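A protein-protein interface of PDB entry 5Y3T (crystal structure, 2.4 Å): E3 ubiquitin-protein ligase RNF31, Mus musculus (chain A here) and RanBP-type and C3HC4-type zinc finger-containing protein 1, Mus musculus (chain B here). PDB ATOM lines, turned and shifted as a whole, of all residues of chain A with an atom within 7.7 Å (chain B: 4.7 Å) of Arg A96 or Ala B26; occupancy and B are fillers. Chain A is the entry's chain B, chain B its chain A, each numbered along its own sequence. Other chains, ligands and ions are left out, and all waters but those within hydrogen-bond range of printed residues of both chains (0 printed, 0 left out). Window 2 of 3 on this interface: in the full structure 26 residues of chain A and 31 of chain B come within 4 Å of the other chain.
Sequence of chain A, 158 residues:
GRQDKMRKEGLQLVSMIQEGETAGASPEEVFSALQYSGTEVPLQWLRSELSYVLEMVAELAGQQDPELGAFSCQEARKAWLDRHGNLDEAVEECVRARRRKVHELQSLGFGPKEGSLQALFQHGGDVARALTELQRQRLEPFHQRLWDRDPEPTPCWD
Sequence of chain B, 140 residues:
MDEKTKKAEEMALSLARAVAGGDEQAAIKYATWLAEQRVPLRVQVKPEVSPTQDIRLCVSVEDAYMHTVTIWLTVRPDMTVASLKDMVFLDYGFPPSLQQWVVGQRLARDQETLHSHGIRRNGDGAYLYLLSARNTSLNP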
ATOM      1  N   ALA A  61     -24.690  -5.455  23.884  1.00  0.00           N
ATOM      2  CA  ALA A  61     -25.265  -6.745  23.515  1.00  0.00           C
ATOM      3  C   ALA A  61     -26.805  -6.661  23.267  1.00  0.00           C
ATOM      4  O   ALA A  61     -27.312  -7.106  22.216  1.00  0.00           O
ATOM      5  CB  ALA A  61     -24.940  -7.759  24.586  1.00  0.00           C
ATOM      6  N   ASP A  65     -28.676  -7.327  19.344  1.00  0.00           N
ATOM      7  CA  ASP A  65     -29.796  -8.232  19.048  1.00  0.00           C
ATOM      8  C   ASP A  65     -30.815  -8.076  20.170  1.00  0.00           C
ATOM      9  O   ASP A  65     -30.696  -8.729  21.203  1.00  0.00           O
ATOM     10  CB  ASP A  65     -29.328  -9.679  18.886  1.00  0.00           C
ATOM     11  CG  ASP A  65     -30.426 -10.613  18.308  1.00  0.00           C
ATOM     12  OD1 ASP A  65     -31.614 -10.243  18.306  1.00  0.00           O
ATOM     13  OD2 ASP A  65     -30.104 -11.741  17.865  1.00  0.00           O
ATOM     14  N   LEU A  68     -32.956 -11.039  22.028  1.00  0.00           N
ATOM     15  CA  LEU A  68     -32.289 -12.016  22.886  1.00  0.00           C
ATOM     16  C   LEU A  68     -32.430 -11.765  24.374  1.00  0.00           C
ATOM     17  O   LEU A  68     -31.797 -12.437  25.209  1.00  0.00           O
ATOM     18  CB  LEU A  68     -30.809 -12.092  22.496  1.00  0.00           C
ATOM     19  CG  LEU A  68     -30.623 -12.768  21.134  1.00  0.00           C
ATOM     20  CD1 LEU A  68     -29.155 -12.789  20.738  1.00  0.00           C
ATOM     21  CD2 LEU A  68     -31.212 -14.175  21.152  1.00  0.00           C
ATOM     22  N   PHE A  71     -28.934  -9.248  28.985  1.00  0.00           N
ATOM     23  CA  PHE A  71     -27.664  -9.890  29.278  1.00  0.00           C
ATOM     24  C   PHE A  71     -27.228  -9.624  30.706  1.00  0.00           C
ATOM     25  O   PHE A  71     -27.372  -8.496  31.215  1.00  0.00           O
ATOM     26  CB  PHE A  71     -26.609  -9.418  28.256  1.00  0.00           C
ATOM     27  CG  PHE A  71     -26.978  -9.786  26.824  1.00  0.00           C
ATOM     28  CD1 PHE A  71     -27.824  -8.978  26.078  1.00  0.00           C
ATOM     29  CD2 PHE A  71     -26.512 -10.977  26.251  1.00  0.00           C
ATOM     30  CE1 PHE A  71     -28.205  -9.335  24.783  1.00  0.00           C
ATOM     31  CE2 PHE A  71     -26.892 -11.348  24.966  1.00  0.00           C
ATOM     32  CZ  PHE A  71     -27.740 -10.530  24.230  1.00  0.00           C
ATOM     33  N   ALA A  79     -17.519 -13.052  28.120  1.00  0.00           N
ATOM     34  CA  ALA A  79     -17.203 -12.592  26.750  1.00  0.00           C
ATOM     35  C   ALA A  79     -16.016 -11.619  26.704  1.00  0.00           C
ATOM     36  O   ALA A  79     -15.077 -11.800  25.942  1.00  0.00           O
ATOM     37  CB  ALA A  79     -18.436 -11.982  26.092  1.00  0.00           C
ATOM     38  N   ASP A  88     -15.429  -4.823  20.906  1.00  0.00           N
ATOM     39  CA  ASP A  88     -16.306  -5.220  19.784  1.00  0.00           C
ATOM     40  C   ASP A  88     -16.366  -6.754  19.653  1.00  0.00           C
ATOM     41  O   ASP A  88     -17.377  -7.312  19.274  1.00  0.00           O
ATOM     42  CB  ASP A  88     -15.855  -4.646  18.421  1.00  0.00           C
ATOM     43  CG  ASP A  88     -16.734  -3.494  17.893  1.00  0.00           C
ATOM     44  OD1 ASP A  88     -17.931  -3.346  18.254  1.00  0.00           O
ATOM     45  OD2 ASP A  88     -16.195  -2.742  17.036  1.00  0.00           O
ATOM     46  N   GLU A  89     -15.287  -7.450  19.928  1.00  0.00           N
ATOM     47  CA  GLU A  89     -15.402  -8.915  19.902  1.00  0.00           C
ATOM     48  C   GLU A  89     -16.200  -9.477  21.068  1.00  0.00           C
ATOM     49  O   GLU A  89     -16.906 -10.467  20.915  1.00  0.00           O
ATOM     50  CB  GLU A  89     -14.045  -9.539  19.838  1.00  0.00           C
ATOM     51  CG  GLU A  89     -13.443  -9.287  18.476  1.00  0.00           C
ATOM     52  CD  GLU A  89     -12.146 -10.008  18.295  1.00  0.00           C
ATOM     53  OE1 GLU A  89     -11.650 -10.695  19.250  1.00  0.00           O
ATOM     54  OE2 GLU A  89     -11.636  -9.857  17.175  1.00  0.00           O
ATOM     55  N   ALA A  90     -16.122  -8.780  22.192  1.00  0.00           N
ATOM     56  CA  ALA A  90     -16.710  -9.211  23.432  1.00  0.00           C
ATOM     57  C   ALA A  90     -18.196  -9.092  23.336  1.00  0.00           C
ATOM     58  O   ALA A  90     -18.932  -9.942  23.842  1.00  0.00           O
ATOM     59  CB  ALA A  90     -16.173  -8.348  24.568  1.00  0.00           C
ATOM     60  N   VAL A  91     -18.618  -8.021  22.671  1.00  0.00           N
ATOM     61  CA  VAL A  91     -20.012  -7.775  22.383  1.00  0.00           C
ATOM     62  C   VAL A  91     -20.523  -8.825  21.420  1.00  0.00           C
ATOM     63  O   VAL A  91     -21.621  -9.336  21.627  1.00  0.00           O
ATOM     64  CB  VAL A  91     -20.249  -6.335  21.821  1.00  0.00           C
ATOM     65  CG1 VAL A  91     -21.647  -6.188  21.204  1.00  0.00           C
ATOM     66  CG2 VAL A  91     -20.070  -5.303  22.934  1.00  0.00           C
ATOM     67  N   GLU A  92     -19.750  -9.123  20.380  1.00  0.00           N
ATOM     68  CA  GLU A  92     -20.102 -10.136  19.384  1.00  0.00           C
ATOM     69  C   GLU A  92     -20.350 -11.449  20.073  1.00  0.00           C
ATOM     70  O   GLU A  92     -21.391 -12.066  19.839  1.00  0.00           O
ATOM     71  CB  GLU A  92     -18.969 -10.362  18.336  1.00  0.00           C
ATOM     72  CG  GLU A  92     -19.086  -9.711  16.945  1.00  0.00           C
ATOM     73  CD  GLU A  92     -17.712  -9.558  16.201  1.00  0.00           C
ATOM     74  OE1 GLU A  92     -16.707 -10.288  16.447  1.00  0.00           O
ATOM     75  OE2 GLU A  92     -17.613  -8.658  15.347  1.00  0.00           O
ATOM     76  N   GLU A  93     -19.384 -11.883  20.900  1.00  0.00           N
ATOM     77  CA  GLU A  93     -19.478 -13.175  21.598  1.00  0.00           C
ATOM     78  C   GLU A  93     -20.525 -13.209  22.682  1.00  0.00           C
ATOM     79  O   GLU A  93     -21.079 -14.263  22.957  1.00  0.00           O
ATOM     80  CB  GLU A  93     -18.113 -13.614  22.211  1.00  0.00           C
ATOM     81  CG  GLU A  93     -17.052 -13.929  21.151  1.00  0.00           C
ATOM     82  CD  GLU A  93     -17.557 -14.788  19.965  1.00  0.00           C
ATOM     83  OE1 GLU A  93     -17.993 -15.920  20.204  1.00  0.00           O
ATOM     84  OE2 GLU A  93     -17.498 -14.361  18.795  1.00  0.00           O
ATOM     85  N   CYS A  94     -20.761 -12.090  23.376  1.00  0.00           N
ATOM     86  CA  CYS A  94     -21.808 -12.068  24.416  1.00  0.00           C
ATOM     87  C   CYS A  94     -23.199 -12.407  23.792  1.00  0.00           C
ATOM     88  O   CYS A  94     -23.952 -13.283  24.265  1.00  0.00           O
ATOM     89  CB  CYS A  94     -21.781 -10.726  25.112  1.00  0.00           C
ATOM     90  SG  CYS A  94     -22.982 -10.546  26.421  1.00  0.00           S
ATOM     91  N   VAL A  95     -23.455 -11.749  22.669  1.00  0.00           N
ATOM     92  CA  VAL A  95     -24.616 -11.957  21.800  1.00  0.00           C
ATOM     93  C   VAL A  95     -24.658 -13.367  21.238  1.00  0.00           C
ATOM     94  O   VAL A  95     -25.712 -14.029  21.271  1.00  0.00           O
ATOM     95  CB  VAL A  95     -24.555 -10.953  20.620  1.00  0.00           C
ATOM     96  CG1 VAL A  95     -25.514 -11.304  19.470  1.00  0.00           C
ATOM     97  CG2 VAL A  95     -24.801  -9.541  21.136  1.00  0.00           C
ATOM     98  N   ARG A  96     -23.521 -13.807  20.702  1.00  0.00           N
ATOM     99  CA  ARG A  96     -23.420 -15.134  20.097  1.00  0.00           C
ATOM    100  C   ARG A  96     -23.585 -16.264  21.092  1.00  0.00           C
ATOM    101  O   ARG A  96     -24.324 -17.199  20.842  1.00  0.00           O
ATOM    102  CB  ARG A  96     -22.097 -15.268  19.342  1.00  0.00           C
ATOM    103  CG  ARG A  96     -22.103 -14.443  18.053  1.00  0.00           C
ATOM    104  CD  ARG A  96     -20.701 -14.223  17.555  1.00  0.00           C
ATOM    105  NE  ARG A  96     -20.684 -13.462  16.333  1.00  0.00           N
ATOM    106  CZ  ARG A  96     -19.639 -13.313  15.519  1.00  0.00           C
ATOM    107  NH1 ARG A  96     -18.474 -13.882  15.759  1.00  0.00           N
ATOM    108  NH2 ARG A  96     -19.786 -12.603  14.420  1.00  0.00           N
ATOM    109  N   ALA A  97     -22.904 -16.185  22.218  1.00  0.00           N
ATOM    110  CA  ALA A  97     -23.106 -17.156  23.305  1.00  0.00           C
ATOM    111  C   ALA A  97     -24.575 -17.307  23.698  1.00  0.00           C
ATOM    112  O   ALA A  97     -25.046 -18.424  23.806  1.00  0.00           O
ATOM    113  CB  ALA A  97     -22.265 -16.837  24.547  1.00  0.00           C
ATOM    114  N   ARG A  98     -25.290 -16.198  23.863  1.00  0.00           N
ATOM    115  CA  ARG A  98     -26.679 -16.268  24.267  1.00  0.00           C
ATOM    116  C   ARG A  98     -27.597 -16.775  23.158  1.00  0.00           C
ATOM    117  O   ARG A  98     -28.501 -17.536  23.439  1.00  0.00           O
ATOM    118  CB  ARG A  98     -27.154 -14.900  24.703  1.00  0.00           C
ATOM    119  CG  ARG A  98     -28.608 -14.879  25.139  1.00  0.00           C
ATOM    120  CD  ARG A  98     -28.822 -15.388  26.576  1.00  0.00           C
ATOM    121  NE  ARG A  98     -29.954 -14.594  26.952  1.00  0.00           N
ATOM    122  CZ  ARG A  98     -30.040 -13.678  27.904  1.00  0.00           C
ATOM    123  NH1 ARG A  98     -29.130 -13.493  28.855  1.00  0.00           N
ATOM    124  NH2 ARG A  98     -31.160 -13.008  27.951  1.00  0.00           N
ATOM    125  N   ARG A  99     -27.397 -16.297  21.923  1.00  0.00           N
ATOM    126  CA  ARG A  99     -28.058 -16.853  20.734  1.00  0.00           C
ATOM    127  C   ARG A  99     -27.908 -18.362  20.614  1.00  0.00           C
ATOM    128  O   ARG A  99     -28.882 -19.064  20.340  1.00  0.00           O
ATOM    129  CB  ARG A  99     -27.556 -16.202  19.434  1.00  0.00           C
ATOM    130  CG  ARG A  99     -28.503 -16.418  18.267  1.00  0.00           C
ATOM    131  CD  ARG A  99     -27.951 -15.911  16.943  1.00  0.00           C
ATOM    132  NE  ARG A  99     -27.957 -14.458  16.918  1.00  0.00           N
ATOM    133  CZ  ARG A  99     -26.926 -13.658  16.627  1.00  0.00           C
ATOM    134  NH1 ARG A  99     -25.710 -14.121  16.293  1.00  0.00           N
ATOM    135  NH2 ARG A  99     -27.115 -12.348  16.674  1.00  0.00           N
ATOM    136  N   ARG A 100     -26.698 -18.855  20.822  1.00  0.00           N
ATOM    137  CA  ARG A 100     -26.410 -20.270  20.689  1.00  0.00           C
ATOM    138  C   ARG A 100     -27.154 -21.065  21.761  1.00  0.00           C
ATOM    139  O   ARG A 100     -27.624 -22.208  21.532  1.00  0.00           O
ATOM    140  CB  ARG A 100     -24.884 -20.473  20.773  1.00  0.00           C
ATOM    141  CG  ARG A 100     -24.402 -21.910  20.660  1.00  0.00           C
ATOM    142  CD  ARG A 100     -22.889 -22.067  20.693  1.00  0.00           C
ATOM    143  NE  ARG A 100     -22.217 -21.326  21.760  1.00  0.00           N
ATOM    144  CZ  ARG A 100     -22.184 -21.675  23.058  1.00  0.00           C
ATOM    145  NH1 ARG A 100     -22.826 -22.765  23.527  1.00  0.00           N
ATOM    146  NH2 ARG A 100     -21.514 -20.900  23.912  1.00  0.00           N
ATOM    147  N   LYS A 101     -27.253 -20.475  22.948  1.00  0.00           N
ATOM    148  CA  LYS A 101     -27.883 -21.166  24.052  1.00  0.00           C
ATOM    149  C   LYS A 101     -29.407 -21.186  23.910  1.00  0.00           C
ATOM    150  O   LYS A 101     -30.023 -22.155  24.261  1.00  0.00           O
ATOM    151  CB  LYS A 101     -27.429 -20.585  25.372  1.00  0.00           C
ATOM    152  CG  LYS A 101     -25.979 -20.894  25.640  1.00  0.00           C
ATOM    153  CD  LYS A 101     -25.452 -20.149  26.841  1.00  0.00           C
ATOM    154  CE  LYS A 101     -23.925 -20.105  26.900  1.00  0.00           C
ATOM    155  NZ  LYS A 101     -23.532 -19.061  27.879  1.00  0.00           N
ATOM    156  N   VAL A 102     -29.990 -20.141  23.354  1.00  0.00           N
ATOM    157  CA  VAL A 102     -31.417 -20.096  23.086  1.00  0.00           C
ATOM    158  C   VAL A 102     -31.806 -21.094  22.003  1.00  0.00           C
ATOM    159  O   VAL A 102     -32.854 -21.744  22.091  1.00  0.00           O
ATOM    160  CB  VAL A 102     -31.868 -18.647  22.744  1.00  0.00           C
ATOM    161  CG1 VAL A 102     -33.213 -18.597  21.990  1.00  0.00           C
ATOM    162  CG2 VAL A 102     -31.891 -17.812  24.036  1.00  0.00           C
ATOM    163  N   SER B  14     -12.269 -16.244  12.710  1.00  0.00           N
ATOM    164  CA  SER B  14     -13.474 -15.410  12.778  1.00  0.00           C
ATOM    165  C   SER B  14     -14.663 -16.063  12.111  1.00  0.00           C
ATOM    166  O   SER B  14     -15.765 -15.954  12.598  1.00  0.00           O
ATOM    167  CB  SER B  14     -13.241 -14.070  12.138  1.00  0.00           C
ATOM    168  OG  SER B  14     -12.245 -13.392  12.851  1.00  0.00           O
ATOM    169  N   ARG B  17     -16.116 -18.601  14.578  1.00  0.00           N
ATOM    170  CA  ARG B  17     -16.896 -17.916  15.637  1.00  0.00           C
ATOM    171  C   ARG B  17     -18.249 -17.385  15.145  1.00  0.00           C
ATOM    172  O   ARG B  17     -19.285 -17.567  15.811  1.00  0.00           O
ATOM    173  CB  ARG B  17     -16.075 -16.789  16.291  1.00  0.00           C
ATOM    174  CG  ARG B  17     -14.941 -17.329  17.147  1.00  0.00           C
ATOM    175  CD  ARG B  17     -14.366 -16.295  18.096  1.00  0.00           C
ATOM    176  NE  ARG B  17     -14.140 -15.024  17.423  1.00  0.00           N
ATOM    177  CZ  ARG B  17     -13.078 -14.721  16.688  1.00  0.00           C
ATOM    178  NH1 ARG B  17     -12.091 -15.590  16.484  1.00  0.00           N
ATOM    179  NH2 ARG B  17     -13.013 -13.532  16.129  1.00  0.00           N
ATOM    180  N   ALA B  18     -18.242 -16.773  13.965  1.00  0.00           N
ATOM    181  CA  ALA B  18     -19.493 -16.402  13.274  1.00  0.00           C
ATOM    182  C   ALA B  18     -20.438 -17.597  13.120  1.00  0.00           C
ATOM    183  O   ALA B  18     -21.636 -17.515  13.409  1.00  0.00           O
ATOM    184  CB  ALA B  18     -19.168 -15.831  11.914  1.00  0.00           C
ATOM    185  N   GLY B  21     -21.734 -18.922  16.460  1.00  0.00           N
ATOM    186  CA  GLY B  21     -22.572 -17.915  17.075  1.00  0.00           C
ATOM    187  C   GLY B  21     -23.808 -17.520  16.304  1.00  0.00           C
ATOM    188  O   GLY B  21     -24.491 -16.530  16.661  1.00  0.00           O
ATOM    189  N   ASP B  23     -24.121 -16.048  13.499  1.00  0.00           N
ATOM    190  CA  ASP B  23     -24.087 -14.750  12.859  1.00  0.00           C
ATOM    191  C   ASP B  23     -23.962 -15.069  11.368  1.00  0.00           C
ATOM    192  O   ASP B  23     -22.855 -15.241  10.839  1.00  0.00           O
ATOM    193  CB  ASP B  23     -22.966 -13.873  13.442  1.00  0.00           C
ATOM    194  CG  ASP B  23     -22.948 -12.492  12.857  1.00  0.00           C
ATOM    195  OD1 ASP B  23     -23.591 -12.273  11.795  1.00  0.00           O
ATOM    196  OD2 ASP B  23     -22.266 -11.610  13.440  1.00  0.00           O
ATOM    197  N   GLU B  24     -25.123 -15.195  10.721  1.00  0.00           N
ATOM    198  CA  GLU B  24     -25.204 -15.481   9.289  1.00  0.00           C
ATOM    199  C   GLU B  24     -24.459 -14.478   8.415  1.00  0.00           C
ATOM    200  O   GLU B  24     -23.694 -14.908   7.552  1.00  0.00           O
ATOM    201  CB  GLU B  24     -26.644 -15.553   8.809  1.00  0.00           C
ATOM    202  CG  GLU B  24     -27.337 -16.849   9.134  1.00  0.00           C
ATOM    203  CD  GLU B  24     -28.827 -16.757   8.857  1.00  0.00           C
ATOM    204  OE1 GLU B  24     -29.625 -16.950   9.804  1.00  0.00           O
ATOM    205  OE2 GLU B  24     -29.195 -16.464   7.698  1.00  0.00           O
ATOM    206  N   GLN B  25     -24.671 -13.170   8.618  1.00  0.00           N
ATOM    207  CA  GLN B  25     -24.003 -12.164   7.741  1.00  0.00           C
ATOM    208  C   GLN B  25     -22.482 -12.160   7.903  1.00  0.00           C
ATOM    209  O   GLN B  25     -21.782 -11.907   6.938  1.00  0.00           O
ATOM    210  CB  GLN B  25     -24.570 -10.729   7.902  1.00  0.00           C
ATOM    211  CG  GLN B  25     -23.828  -9.581   7.145  1.00  0.00           C
ATOM    212  CD  GLN B  25     -23.986  -9.573   5.595  1.00  0.00           C
ATOM    213  OE1 GLN B  25     -23.030  -9.828   4.840  1.00  0.00           O
ATOM    214  NE2 GLN B  25     -25.191  -9.254   5.125  1.00  0.00           N
ATOM    215  N   ALA B  26     -21.973 -12.424   9.105  1.00  0.00           N
ATOM    216  CA  ALA B  26     -20.522 -12.428   9.327  1.00  0.00           C
ATOM    217  C   ALA B  26     -19.933 -13.742   8.752  1.00  0.00           C
ATOM    218  O   ALA B  26     -18.884 -13.741   8.116  1.00  0.00           O
ATOM    219  CB  ALA B  26     -20.198 -12.250  10.810  1.00  0.00           C
ATOM    220  N   ALA B  27     -20.637 -14.845   8.934  1.00  0.00           N
ATOM    221  CA  ALA B  27     -20.212 -16.091   8.304  1.00  0.00           C
ATOM    222  C   ALA B  27     -20.049 -15.908   6.793  1.00  0.00           C
ATOM    223  O   ALA B  27     -19.081 -16.395   6.227  1.00  0.00           O
ATOM    224  CB  ALA B  27     -21.171 -17.219   8.611  1.00  0.00           C
ATOM    225  N   ILE B  28     -20.969 -15.161   6.175  1.00  0.00           N
ATOM    226  CA  ILE B  28     -20.921 -14.873   4.736  1.00  0.00           C
ATOM    227  C   ILE B  28     -19.700 -14.021   4.399  1.00  0.00           C
ATOM    228  O   ILE B  28     -18.994 -14.323   3.430  1.00  0.00           O
ATOM    229  CB  ILE B  28     -22.184 -14.166   4.213  1.00  0.00           C
ATOM    230  CG1 ILE B  28     -23.380 -15.102   4.253  1.00  0.00           C
ATOM    231  CG2 ILE B  28     -21.990 -13.698   2.773  1.00  0.00           C
ATOM    232  CD1 ILE B  28     -24.699 -14.419   3.916  1.00  0.00           C
ATOM    233  N   LYS B  29     -19.455 -12.987   5.198  1.00  0.00           N
ATOM    234  CA  LYS B  29     -18.321 -12.125   4.960  1.00  0.00           C
ATOM    235  C   LYS B  29     -16.955 -12.825   4.985  1.00  0.00           C
ATOM    236  O   LYS B  29     -16.120 -12.591   4.121  1.00  0.00           O
ATOM    237  CB  LYS B  29     -18.298 -11.000   5.961  1.00  0.00           C
ATOM    238  CG  LYS B  29     -17.215  -9.975   5.687  1.00  0.00           C
ATOM    239  CD  LYS B  29     -17.324  -8.807   6.664  1.00  0.00           C
ATOM    240  CE  LYS B  29     -16.838  -9.150   8.058  1.00  0.00           C
ATOM    241  NZ  LYS B  29     -16.409  -7.932   8.814  1.00  0.00           N
ATOM    242  N   TYR B  30     -16.719 -13.634   6.006  1.00  0.00           N
ATOM    243  CA  TYR B  30     -15.430 -14.274   6.169  1.00  0.00           C
ATOM    244  C   TYR B  30     -15.267 -15.394   5.157  1.00  0.00           C
ATOM    245  O   TYR B  30     -14.208 -15.536   4.608  1.00  0.00           O
ATOM    246  CB  TYR B  30     -15.244 -14.778   7.623  1.00  0.00           C
ATOM    247  CG  TYR B  30     -15.254 -13.654   8.646  1.00  0.00           C
ATOM    248  CD1 TYR B  30     -14.334 -12.616   8.559  1.00  0.00           C
ATOM    249  CD2 TYR B  30     -16.198 -13.620   9.692  1.00  0.00           C
ATOM    250  CE1 TYR B  30     -14.341 -11.579   9.480  1.00  0.00           C
ATOM    251  CE2 TYR B  30     -16.234 -12.568  10.619  1.00  0.00           C
ATOM    252  CZ  TYR B  30     -15.298 -11.554  10.512  1.00  0.00           C
ATOM    253  OH  TYR B  30     -15.263 -10.528  11.427  1.00  0.00           O
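The guanidinium group (NH1) of Arg A96 sits close to the backbone NH (N) of Ala B18, 3.4 Å away. OD2 of Asp B23 is in salt-bridge range of NH2 of Arg A96 (2.8 Å). The guanidinium group of Arg A99 is in hydrogen-bond range of the backbone carbonyl oxygen of Gly B21, at 2.7 Å. NE of Arg B17 lies within salt-bridge range of OE2 of Glu A93, at 3.7 Å.
The backbone carbonyl oxygen (O) of Ala B18 lies within hydrogen-bond range of the backbone NH (N) of Asp B23 (2.9 Å). The side-chain hydroxyl (OG) of Ser B14 lies within hydrogen-bond range of the guanidinium group (NH2) of Arg B17 (3.4 Å). The backbone NH (N) of Ala B26 sits at hydrogen-bond distance from the side-chain carboxylate (OD1) of Asp B23 (3.1 Å). NH2 of Arg A99 is in salt-bridge range of OD2 of Asp A65, 3.3 Å away. The guanidinium group (NH1) of Arg A96 is in salt-bridge range of the side-chain carboxylate (OE2) of Glu A93, at 3.2 Å. The side-chain carboxylate (OD1) of Asp B23 lies close to the backbone NH (N) of Gln B25 (3.5 Å).
Arg A96 touches Arg B17. Arg A96 touches Gly B21 (CG to O, 3.5 Å). Ala B26 touches Arg A96. Asp B23 touches Arg A99.
Ala B26 touches just one residue of chain A: Arg A96 (3.7 Å). Of the printed residues of chain A, Arg B17 touches Glu A93 (3.7 Å) and Arg A96 (3.6 Å). Printed residues of chain A within 4 Å of Asp B23: Arg A96 and Arg A99. Of the printed residues of chain B, Arg A99 touches Gly B21 and Asp B23. Printed residues of chain A within 4 Å of Ala B18: Arg A96. Val A102 touches none of the printed residues of chain B. The nearest printed residue of chain B that does not touch Arg A96 is Ser B14 (4.7 Å).
Of the 20 printed residues of chain A, 3 touch a printed residue of chain B. Printed residues of chain B that touch a printed residue of chain A: Arg B17, Ala B18, Gly B21, Asp B23 and Ala B26.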
